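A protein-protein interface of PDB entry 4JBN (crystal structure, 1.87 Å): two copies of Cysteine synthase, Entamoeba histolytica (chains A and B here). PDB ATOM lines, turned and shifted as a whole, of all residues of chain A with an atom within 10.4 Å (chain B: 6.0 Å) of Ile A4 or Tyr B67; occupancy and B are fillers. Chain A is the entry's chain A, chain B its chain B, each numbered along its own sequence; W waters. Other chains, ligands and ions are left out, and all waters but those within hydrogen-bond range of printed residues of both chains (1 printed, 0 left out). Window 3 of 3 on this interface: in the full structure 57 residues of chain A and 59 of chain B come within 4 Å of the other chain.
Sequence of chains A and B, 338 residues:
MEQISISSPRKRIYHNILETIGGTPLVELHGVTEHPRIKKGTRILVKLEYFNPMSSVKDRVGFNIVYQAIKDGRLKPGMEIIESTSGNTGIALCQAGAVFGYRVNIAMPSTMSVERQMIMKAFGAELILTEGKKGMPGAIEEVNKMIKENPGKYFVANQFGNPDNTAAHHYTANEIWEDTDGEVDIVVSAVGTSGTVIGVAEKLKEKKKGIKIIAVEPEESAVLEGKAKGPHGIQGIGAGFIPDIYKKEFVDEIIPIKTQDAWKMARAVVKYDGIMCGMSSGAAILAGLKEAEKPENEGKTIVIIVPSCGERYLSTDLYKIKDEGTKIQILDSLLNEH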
ATOM      1  N   GLU A   2     -19.355 -21.903 -18.771  1.00  0.00           N
ATOM      2  CA  GLU A   2     -19.013 -23.259 -18.410  1.00  0.00           C
ATOM      3  C   GLU A   2     -18.406 -23.365 -17.024  1.00  0.00           C
ATOM      4  O   GLU A   2     -18.590 -24.371 -16.338  1.00  0.00           O
ATOM      5  CB  GLU A   2     -18.109 -23.855 -19.462  1.00  0.00           C
ATOM      6  CG  GLU A   2     -17.867 -25.336 -19.323  1.00  0.00           C
ATOM      7  CD  GLU A   2     -16.486 -25.604 -18.809  1.00  0.00           C
ATOM      8  OE1 GLU A   2     -15.893 -24.661 -18.292  1.00  0.00           O
ATOM      9  OE2 GLU A   2     -16.022 -26.748 -18.901  1.00  0.00           O
ATOM     10  N   GLN A   3     -17.680 -22.318 -16.640  1.00  0.00           N
ATOM     11  CA  GLN A   3     -17.384 -21.990 -15.270  1.00  0.00           C
ATOM     12  C   GLN A   3     -18.725 -21.766 -14.584  1.00  0.00           C
ATOM     13  O   GLN A   3     -19.605 -21.149 -15.149  1.00  0.00           O
ATOM     14  CB  GLN A   3     -16.566 -20.696 -15.225  1.00  0.00           C
ATOM     15  CG  GLN A   3     -16.949 -19.664 -16.298  1.00  0.00           C
ATOM     16  CD  GLN A   3     -15.847 -18.674 -16.639  1.00  0.00           C
ATOM     17  OE1 GLN A   3     -15.936 -17.502 -16.313  1.00  0.00           O
ATOM     18  NE2 GLN A   3     -14.813 -19.143 -17.317  1.00  0.00           N
ATOM     19  N   ILE A   4     -18.877 -22.292 -13.375  1.00  0.00           N
ATOM     20  CA  ILE A   4     -20.064 -22.046 -12.575  1.00  0.00           C
ATOM     21  C   ILE A   4     -19.737 -21.421 -11.235  1.00  0.00           C
ATOM     22  O   ILE A   4     -19.101 -22.031 -10.431  1.00  0.00           O
ATOM     23  CB  ILE A   4     -20.873 -23.309 -12.321  1.00  0.00           C
ATOM     24  CG1 ILE A   4     -21.365 -23.896 -13.603  1.00  0.00           C
ATOM     25  CG2 ILE A   4     -22.167 -22.987 -11.635  1.00  0.00           C
ATOM     26  CD1 ILE A   4     -22.745 -24.444 -13.440  1.00  0.00           C
ATOM     27  N   SER A   5     -20.203 -20.205 -11.008  1.00  0.00           N
ATOM     28  CA  SER A   5     -19.898 -19.488  -9.745  1.00  0.00           C
ATOM     29  C   SER A   5     -21.158 -19.478  -8.955  1.00  0.00           C
ATOM     30  O   SER A   5     -22.221 -19.073  -9.477  1.00  0.00           O
ATOM     31  CB  SER A   5     -19.551 -18.031 -10.015  1.00  0.00           C
ATOM     32  OG  SER A   5     -18.517 -17.971 -10.976  1.00  0.00           O
ATOM     33  N   ILE A   6     -21.084 -19.985  -7.743  1.00  0.00           N
ATOM     34  CA  ILE A   6     -22.227 -19.817  -6.829  1.00  0.00           C
ATOM     35  C   ILE A   6     -22.342 -18.397  -6.311  1.00  0.00           C
ATOM     36  O   ILE A   6     -21.506 -17.539  -6.639  1.00  0.00           O
ATOM     37  CB  ILE A   6     -22.194 -20.843  -5.677  1.00  0.00           C
ATOM     38  CG1 ILE A   6     -20.954 -20.654  -4.766  1.00  0.00           C
ATOM     39  CG2 ILE A   6     -22.409 -22.241  -6.285  1.00  0.00           C
ATOM     40  CD1 ILE A   6     -21.174 -21.315  -3.376  1.00  0.00           C
ATOM     41  N   SER A   7     -23.325 -18.128  -5.464  1.00  0.00           N
ATOM     42  CA  SER A   7     -23.531 -16.718  -4.981  1.00  0.00           C
ATOM     43  C   SER A   7     -22.523 -16.305  -3.966  1.00  0.00           C
ATOM     44  O   SER A   7     -22.087 -17.122  -3.153  1.00  0.00           O
ATOM     45  CB  SER A   7     -24.937 -16.510  -4.399  1.00  0.00           C
ATOM     46  OG  SER A   7     -25.873 -16.837  -5.448  1.00  0.00           O
ATOM     47  N   SER A   8     -22.176 -15.012  -3.992  1.00  0.00           N
ATOM     48  CA  SER A   8     -21.243 -14.418  -3.069  1.00  0.00           C
ATOM     49  C   SER A   8     -21.981 -14.047  -1.777  1.00  0.00           C
ATOM     50  O   SER A   8     -23.215 -13.985  -1.779  1.00  0.00           O
ATOM     51  CB  SER A   8     -20.771 -13.046  -3.648  1.00  0.00           C
ATOM     52  OG  SER A   8     -19.935 -13.351  -4.741  1.00  0.00           O
ATOM     53  N   HIS A  30     -33.057 -22.177 -20.064  1.00  0.00           N
ATOM     54  CA  HIS A  30     -32.317 -22.710 -21.227  1.00  0.00           C
ATOM     55  C   HIS A  30     -32.897 -23.991 -21.756  1.00  0.00           C
ATOM     56  O   HIS A  30     -32.930 -24.232 -22.987  1.00  0.00           O
ATOM     57  CB  HIS A  30     -30.834 -22.977 -20.845  1.00  0.00           C
ATOM     58  CG  HIS A  30     -30.062 -21.725 -20.590  1.00  0.00           C
ATOM     59  ND1 HIS A  30     -29.610 -20.876 -21.594  1.00  0.00           N
ATOM     60  CD2 HIS A  30     -29.651 -21.173 -19.414  1.00  0.00           C
ATOM     61  CE1 HIS A  30     -28.990 -19.838 -21.052  1.00  0.00           C
ATOM     62  NE2 HIS A  30     -28.963 -20.015 -19.732  1.00  0.00           N
ATOM     63  N   ARG B  12     -27.707  -9.120 -10.718  1.00  0.00           N
ATOM     64  CA  ARG B  12     -27.014 -10.321 -11.306  1.00  0.00           C
ATOM     65  C   ARG B  12     -28.150 -10.944 -12.109  1.00  0.00           C
ATOM     66  O   ARG B  12     -29.316 -10.859 -11.694  1.00  0.00           O
ATOM     67  CB  ARG B  12     -26.407 -11.322 -10.228  1.00  0.00           C
ATOM     68  CG  ARG B  12     -25.452 -12.449 -10.832  1.00  0.00           C
ATOM     69  CD  ARG B  12     -24.614 -13.409  -9.912  1.00  0.00           C
ATOM     70  NE  ARG B  12     -24.040 -14.572 -10.675  1.00  0.00           N
ATOM     71  CZ  ARG B  12     -23.551 -15.710 -10.135  1.00  0.00           C
ATOM     72  NH1 ARG B  12     -23.590 -16.030  -8.786  1.00  0.00           N
ATOM     73  NH2 ARG B  12     -23.011 -16.603 -10.964  1.00  0.00           N
ATOM     74  N   ASN B  16     -28.131 -20.141 -14.539  1.00  0.00           N
ATOM     75  CA  ASN B  16     -28.948 -21.297 -14.238  1.00  0.00           C
ATOM     76  C   ASN B  16     -29.130 -21.329 -12.733  1.00  0.00           C
ATOM     77  O   ASN B  16     -28.544 -20.493 -12.030  1.00  0.00           O
ATOM     78  CB  ASN B  16     -28.286 -22.595 -14.742  1.00  0.00           C
ATOM     79  CG  ASN B  16     -26.929 -22.806 -14.146  1.00  0.00           C
ATOM     80  OD1 ASN B  16     -26.765 -22.784 -12.902  1.00  0.00           O
ATOM     81  ND2 ASN B  16     -25.881 -22.910 -15.021  1.00  0.00           N
ATOM     82  N   LEU B  18     -28.210 -23.253 -10.382  1.00  0.00           N
ATOM     83  CA  LEU B  18     -27.091 -23.564  -9.494  1.00  0.00           C
ATOM     84  C   LEU B  18     -26.328 -22.364  -9.099  1.00  0.00           C
ATOM     85  O   LEU B  18     -25.721 -22.356  -8.049  1.00  0.00           O
ATOM     86  CB  LEU B  18     -26.119 -24.587 -10.203  1.00  0.00           C
ATOM     87  CG  LEU B  18     -26.808 -25.900 -10.636  1.00  0.00           C
ATOM     88  CD1 LEU B  18     -25.746 -26.788 -11.327  1.00  0.00           C
ATOM     89  CD2 LEU B  18     -27.569 -26.703  -9.553  1.00  0.00           C
ATOM     90  N   GLU B  19     -26.334 -21.290  -9.923  1.00  0.00           N
ATOM     91  CA  GLU B  19     -25.617 -20.112  -9.498  1.00  0.00           C
ATOM     92  C   GLU B  19     -26.321 -19.366  -8.352  1.00  0.00           C
ATOM     93  O   GLU B  19     -25.695 -18.448  -7.801  1.00  0.00           O
ATOM     94  CB  GLU B  19     -25.446 -19.132 -10.670  1.00  0.00           C
ATOM     95  CG  GLU B  19     -24.565 -19.775 -11.776  1.00  0.00           C
ATOM     96  CD  GLU B  19     -24.193 -18.774 -12.881  1.00  0.00           C
ATOM     97  OE1 GLU B  19     -24.928 -17.855 -13.158  1.00  0.00           O
ATOM     98  OE2 GLU B  19     -23.183 -18.976 -13.538  1.00  0.00           O
ATOM     99  N   GLY B  62     -24.769 -31.306  -3.014  1.00  0.00           N
ATOM    100  CA  GLY B  62     -25.063 -31.902  -4.307  1.00  0.00           C
ATOM    101  C   GLY B  62     -24.406 -31.168  -5.457  1.00  0.00           C
ATOM    102  O   GLY B  62     -23.786 -31.794  -6.358  1.00  0.00           O
ATOM    103  N   PHE B  63     -24.426 -29.839  -5.398  1.00  0.00           N
ATOM    104  CA  PHE B  63     -23.713 -29.105  -6.414  1.00  0.00           C
ATOM    105  C   PHE B  63     -22.208 -29.414  -6.459  1.00  0.00           C
ATOM    106  O   PHE B  63     -21.639 -29.649  -7.532  1.00  0.00           O
ATOM    107  CB  PHE B  63     -23.896 -27.596  -6.256  1.00  0.00           C
ATOM    108  CG  PHE B  63     -22.991 -26.799  -7.151  1.00  0.00           C
ATOM    109  CD1 PHE B  63     -23.195 -26.809  -8.535  1.00  0.00           C
ATOM    110  CD2 PHE B  63     -21.875 -26.173  -6.656  1.00  0.00           C
ATOM    111  CE1 PHE B  63     -22.344 -26.099  -9.381  1.00  0.00           C
ATOM    112  CE2 PHE B  63     -21.007 -25.467  -7.497  1.00  0.00           C
ATOM    113  CZ  PHE B  63     -21.250 -25.428  -8.850  1.00  0.00           C
ATOM    114  N   ASN B  64     -21.546 -29.265  -5.327  1.00  0.00           N
ATOM    115  CA  ASN B  64     -20.082 -29.331  -5.395  1.00  0.00           C
ATOM    116  C   ASN B  64     -19.596 -30.773  -5.651  1.00  0.00           C
ATOM    117  O   ASN B  64     -18.566 -30.966  -6.306  1.00  0.00           O
ATOM    118  CB  ASN B  64     -19.441 -28.887  -4.088  1.00  0.00           C
ATOM    119  CG  ASN B  64     -18.024 -28.447  -4.299  1.00  0.00           C
ATOM    120  OD1 ASN B  64     -17.764 -27.751  -5.307  1.00  0.00           O
ATOM    121  ND2 ASN B  64     -17.068 -28.881  -3.424  1.00  0.00           N
ATOM    122  N   ILE B  65     -20.277 -31.752  -5.083  1.00  0.00           N
ATOM    123  CA  ILE B  65     -19.964 -33.170  -5.423  1.00  0.00           C
ATOM    124  C   ILE B  65     -19.992 -33.405  -6.941  1.00  0.00           C
ATOM    125  O   ILE B  65     -19.045 -34.009  -7.542  1.00  0.00           O
ATOM    126  CB  ILE B  65     -20.896 -34.143  -4.673  1.00  0.00           C
ATOM    127  CG1 ILE B  65     -20.470 -34.131  -3.138  1.00  0.00           C
ATOM    128  CG2 ILE B  65     -20.825 -35.557  -5.310  1.00  0.00           C
ATOM    129  CD1 ILE B  65     -21.341 -35.014  -2.249  1.00  0.00           C
ATOM    130  N   VAL B  66     -21.073 -32.976  -7.557  1.00  0.00           N
ATOM    131  CA  VAL B  66     -21.267 -33.240  -9.004  1.00  0.00           C
ATOM    132  C   VAL B  66     -20.330 -32.353  -9.834  1.00  0.00           C
ATOM    133  O   VAL B  66     -19.588 -32.814 -10.785  1.00  0.00           O
ATOM    134  CB  VAL B  66     -22.757 -33.071  -9.359  1.00  0.00           C
ATOM    135  CG1 VAL B  66     -22.977 -33.112 -10.880  1.00  0.00           C
ATOM    136  CG2 VAL B  66     -23.581 -34.202  -8.706  1.00  0.00           C
ATOM    137  N   TYR B  67     -20.281 -31.088  -9.516  1.00  0.00           N
ATOM    138  CA  TYR B  67     -19.353 -30.183 -10.175  1.00  0.00           C
ATOM    139  C   TYR B  67     -17.856 -30.581 -10.115  1.00  0.00           C
ATOM    140  O   TYR B  67     -17.192 -30.627 -11.096  1.00  0.00           O
ATOM    141  CB  TYR B  67     -19.518 -28.817  -9.597  1.00  0.00           C
ATOM    142  CG  TYR B  67     -18.755 -27.744 -10.257  1.00  0.00           C
ATOM    143  CD1 TYR B  67     -18.956 -27.437 -11.564  1.00  0.00           C
ATOM    144  CD2 TYR B  67     -17.888 -26.987  -9.549  1.00  0.00           C
ATOM    145  CE1 TYR B  67     -18.258 -26.435 -12.167  1.00  0.00           C
ATOM    146  CE2 TYR B  67     -17.187 -25.966 -10.133  1.00  0.00           C
ATOM    147  CZ  TYR B  67     -17.388 -25.700 -11.451  1.00  0.00           C
ATOM    148  OH  TYR B  67     -16.711 -24.697 -12.026  1.00  0.00           O
ATOM    149  N   GLN B  68     -17.351 -30.836  -8.935  1.00  0.00           N
ATOM    150  CA  GLN B  68     -15.970 -31.260  -8.805  1.00  0.00           C
ATOM    151  C   GLN B  68     -15.669 -32.585  -9.508  1.00  0.00           C
ATOM    152  O   GLN B  68     -14.610 -32.783 -10.033  1.00  0.00           O
ATOM    153  CB  GLN B  68     -15.552 -31.308  -7.357  1.00  0.00           C
ATOM    154  CG  GLN B  68     -15.708 -30.035  -6.609  1.00  0.00           C
ATOM    155  CD  GLN B  68     -14.800 -28.915  -7.075  1.00  0.00           C
ATOM    156  OE1 GLN B  68     -13.718 -29.140  -7.522  1.00  0.00           O
ATOM    157  NE2 GLN B  68     -15.264 -27.686  -6.912  1.00  0.00           N
ATOM    158  N   ALA B  69     -16.617 -33.492  -9.497  1.00  0.00           N
ATOM    159  CA  ALA B  69     -16.404 -34.767 -10.206  1.00  0.00           C
ATOM    160  C   ALA B  69     -16.374 -34.553 -11.736  1.00  0.00           C
ATOM    161  O   ALA B  69     -15.623 -35.238 -12.467  1.00  0.00           O
ATOM    162  CB  ALA B  69     -17.470 -35.754  -9.848  1.00  0.00           C
ATOM    163  N   ILE B  70     -17.208 -33.627 -12.223  1.00  0.00           N
ATOM    164  CA  ILE B  70     -17.151 -33.296 -13.618  1.00  0.00           C
ATOM    165  C   ILE B  70     -15.796 -32.672 -13.891  1.00  0.00           C
ATOM    166  O   ILE B  70     -15.165 -33.048 -14.854  1.00  0.00           O
ATOM    167  CB  ILE B  70     -18.329 -32.421 -14.089  1.00  0.00           C
ATOM    168  CG1 ILE B  70     -19.599 -33.252 -14.116  1.00  0.00           C
ATOM    169  CG2 ILE B  70     -18.002 -31.783 -15.445  1.00  0.00           C
ATOM    170  CD1 ILE B  70     -20.883 -32.432 -14.260  1.00  0.00           C
ATOM    171  N   LYS B  71     -15.329 -31.741 -13.080  1.00  0.00           N
ATOM    172  CA  LYS B  71     -14.074 -31.076 -13.346  1.00  0.00           C
ATOM    173  C   LYS B  71     -12.874 -32.030 -13.297  1.00  0.00           C
ATOM    174  O   LYS B  71     -11.939 -31.842 -14.121  1.00  0.00           O
ATOM    175  CB  LYS B  71     -13.821 -29.929 -12.405  1.00  0.00           C
ATOM    176  CG  LYS B  71     -14.584 -28.679 -12.827  1.00  0.00           C
ATOM    177  CD  LYS B  71     -14.671 -27.687 -11.680  1.00  0.00           C
ATOM    178  CE  LYS B  71     -13.315 -27.328 -11.104  1.00  0.00           C
ATOM    179  NZ  LYS B  71     -13.586 -26.860  -9.710  1.00  0.00           N
ATOM    180  N   ASP B  72     -12.906 -32.969 -12.348  1.00  0.00           N
ATOM    181  CA  ASP B  72     -11.864 -34.029 -12.126  1.00  0.00           C
ATOM    182  C   ASP B  72     -11.815 -35.109 -13.159  1.00  0.00           C
ATOM    183  O   ASP B  72     -10.805 -35.858 -13.189  1.00  0.00           O
ATOM    184  CB  ASP B  72     -12.178 -34.840 -10.805  1.00  0.00           C
ATOM    185  CG  ASP B  72     -11.732 -34.103  -9.611  1.00  0.00           C
ATOM    186  OD1 ASP B  72     -11.409 -32.896  -9.803  1.00  0.00           O
ATOM    187  OD2 ASP B  72     -11.677 -34.701  -8.503  1.00  0.00           O
ATOM    188  N   VAL B  99     -29.474 -29.891 -14.179  1.00  0.00           N
ATOM    189  CA  VAL B  99     -28.816 -28.800 -14.852  1.00  0.00           C
ATOM    190  C   VAL B  99     -27.614 -29.285 -15.627  1.00  0.00           C
ATOM    191  O   VAL B  99     -27.398 -28.837 -16.738  1.00  0.00           O
ATOM    192  CB  VAL B  99     -28.361 -27.737 -13.824  1.00  0.00           C
ATOM    193  CG1 VAL B  99     -27.482 -26.634 -14.452  1.00  0.00           C
ATOM    194  CG2 VAL B  99     -29.610 -27.207 -13.172  1.00  0.00           C
ATOM    195  N   PHE B 100     -26.826 -30.182 -15.068  1.00  0.00           N
ATOM    196  CA  PHE B 100     -25.663 -30.647 -15.788  1.00  0.00           C
ATOM    197  C   PHE B 100     -26.024 -31.660 -16.869  1.00  0.00           C
ATOM    198  O   PHE B 100     -25.225 -31.944 -17.685  1.00  0.00           O
ATOM    199  CB  PHE B 100     -24.635 -31.236 -14.861  1.00  0.00           C
ATOM    200  CG  PHE B 100     -23.876 -30.248 -14.079  1.00  0.00           C
ATOM    201  CD1 PHE B 100     -23.085 -29.335 -14.681  1.00  0.00           C
ATOM    202  CD2 PHE B 100     -23.922 -30.268 -12.736  1.00  0.00           C
ATOM    203  CE1 PHE B 100     -22.366 -28.447 -13.931  1.00  0.00           C
ATOM    204  CE2 PHE B 100     -23.243 -29.391 -11.998  1.00  0.00           C
ATOM    205  CZ  PHE B 100     -22.444 -28.484 -12.580  1.00  0.00           C
HETATM  206  O   HOH W   1     -22.717 -21.101 -15.050  1.00  0.00           O
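Water W1 bridges OE2 of Glu B19 (2.6 Å) and O of Gln A3 (3.1 Å).
Of the printed residues of chain B, Ile A4 touches Asn B16, Phe B63 and Tyr B67. No residue of chain A comes within 4 Å of Gln B68. No residue of chain A comes within 4 Å of Ala B69. No residue of chain A comes within 4 Å of Ile B70. Lys B71 touches none of the printed residues of chain A. Printed residues of chain B within 4 Å of Ile A6: Arg B12 (3.4 Å), Leu B18 (3.8 Å), Glu B19 (3.7 Å) and Phe B63 (3.7 Å). Of the printed residues of chain B, Ser A5 touches Arg B12 and Glu B19. Of the printed residues of chain A, Arg B12 touches Ser A5 (3.0 Å), Ile A6 (3.4 Å) and Ser A7 (3.9 Å). Of the printed residues of chain B, Ser A7 touches Arg B12 (3.9 Å) and Glu B19 (2.9 Å). Of the printed residues of chain A, Asn B16 touches Ile A4. Phe B100 touches none of the printed residues of chain A. Ser A8 touches none of the printed residues of chain B. The nearest printed residue of chain B that does not touch Ile A4 is Glu B19 (4.01 Å).
No position is printed for both chains.
Of the 17 printed residues of chain B, 6 touch a printed residue of chain A. Printed residues of chain B that touch a printed residue of chain A: Arg B12, Asn B16, Leu B18, Glu B19, Phe B63 and Tyr B67. Printed residues of chain A that touch a printed residue of chain B: Ile A4, Ser A5, Ile A6 and Ser A7. Hydrophobic or aromatic side chains of chain A that line the printed part of chain B: Ile A4 and Ile A6. Among the printed residues, 11 pairs touch across the chains. Among the printed residues, no Asp or Glu carboxylate lies within 4 Å of a Lys or Arg side-chain nitrogen of the other chain.
The guanidinium group (NH2) of Arg B12 lies within hydrogen-bond range of the backbone carbonyl oxygen (O) of Ser A5 (3.0 Å). The side-chain hydroxyl of Ser A7 sits at hydrogen-bond distance from the backbone carbonyl oxygen of Glu B19 (2.9 Å). O of Ile A6 sits at hydrogen-bond distance from NH1 of Arg B12.
Among the printed residues, merely in contact across the chains: Ser A5 with Glu B19, Ile A4 with Tyr B67, Ile A6 with Glu B19, Ile A6 with Phe B63, Ile A6 with Leu B18, Ile A4 with Phe B63, Ile A4 with Asn B16 and Ser A7 with Arg B12.
The side-chain amide oxygen of Asn B16 sits at hydrogen-bond distance from the backbone NH of Leu B18, 2.9 Å away. OE1 of Glu B19 is in salt-bridge range of NH2 of Arg B12. The backbone NH of Glu B19 lies within hydrogen-bond range of the side-chain amide oxygen of Asn B16, 3.4 Å away.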
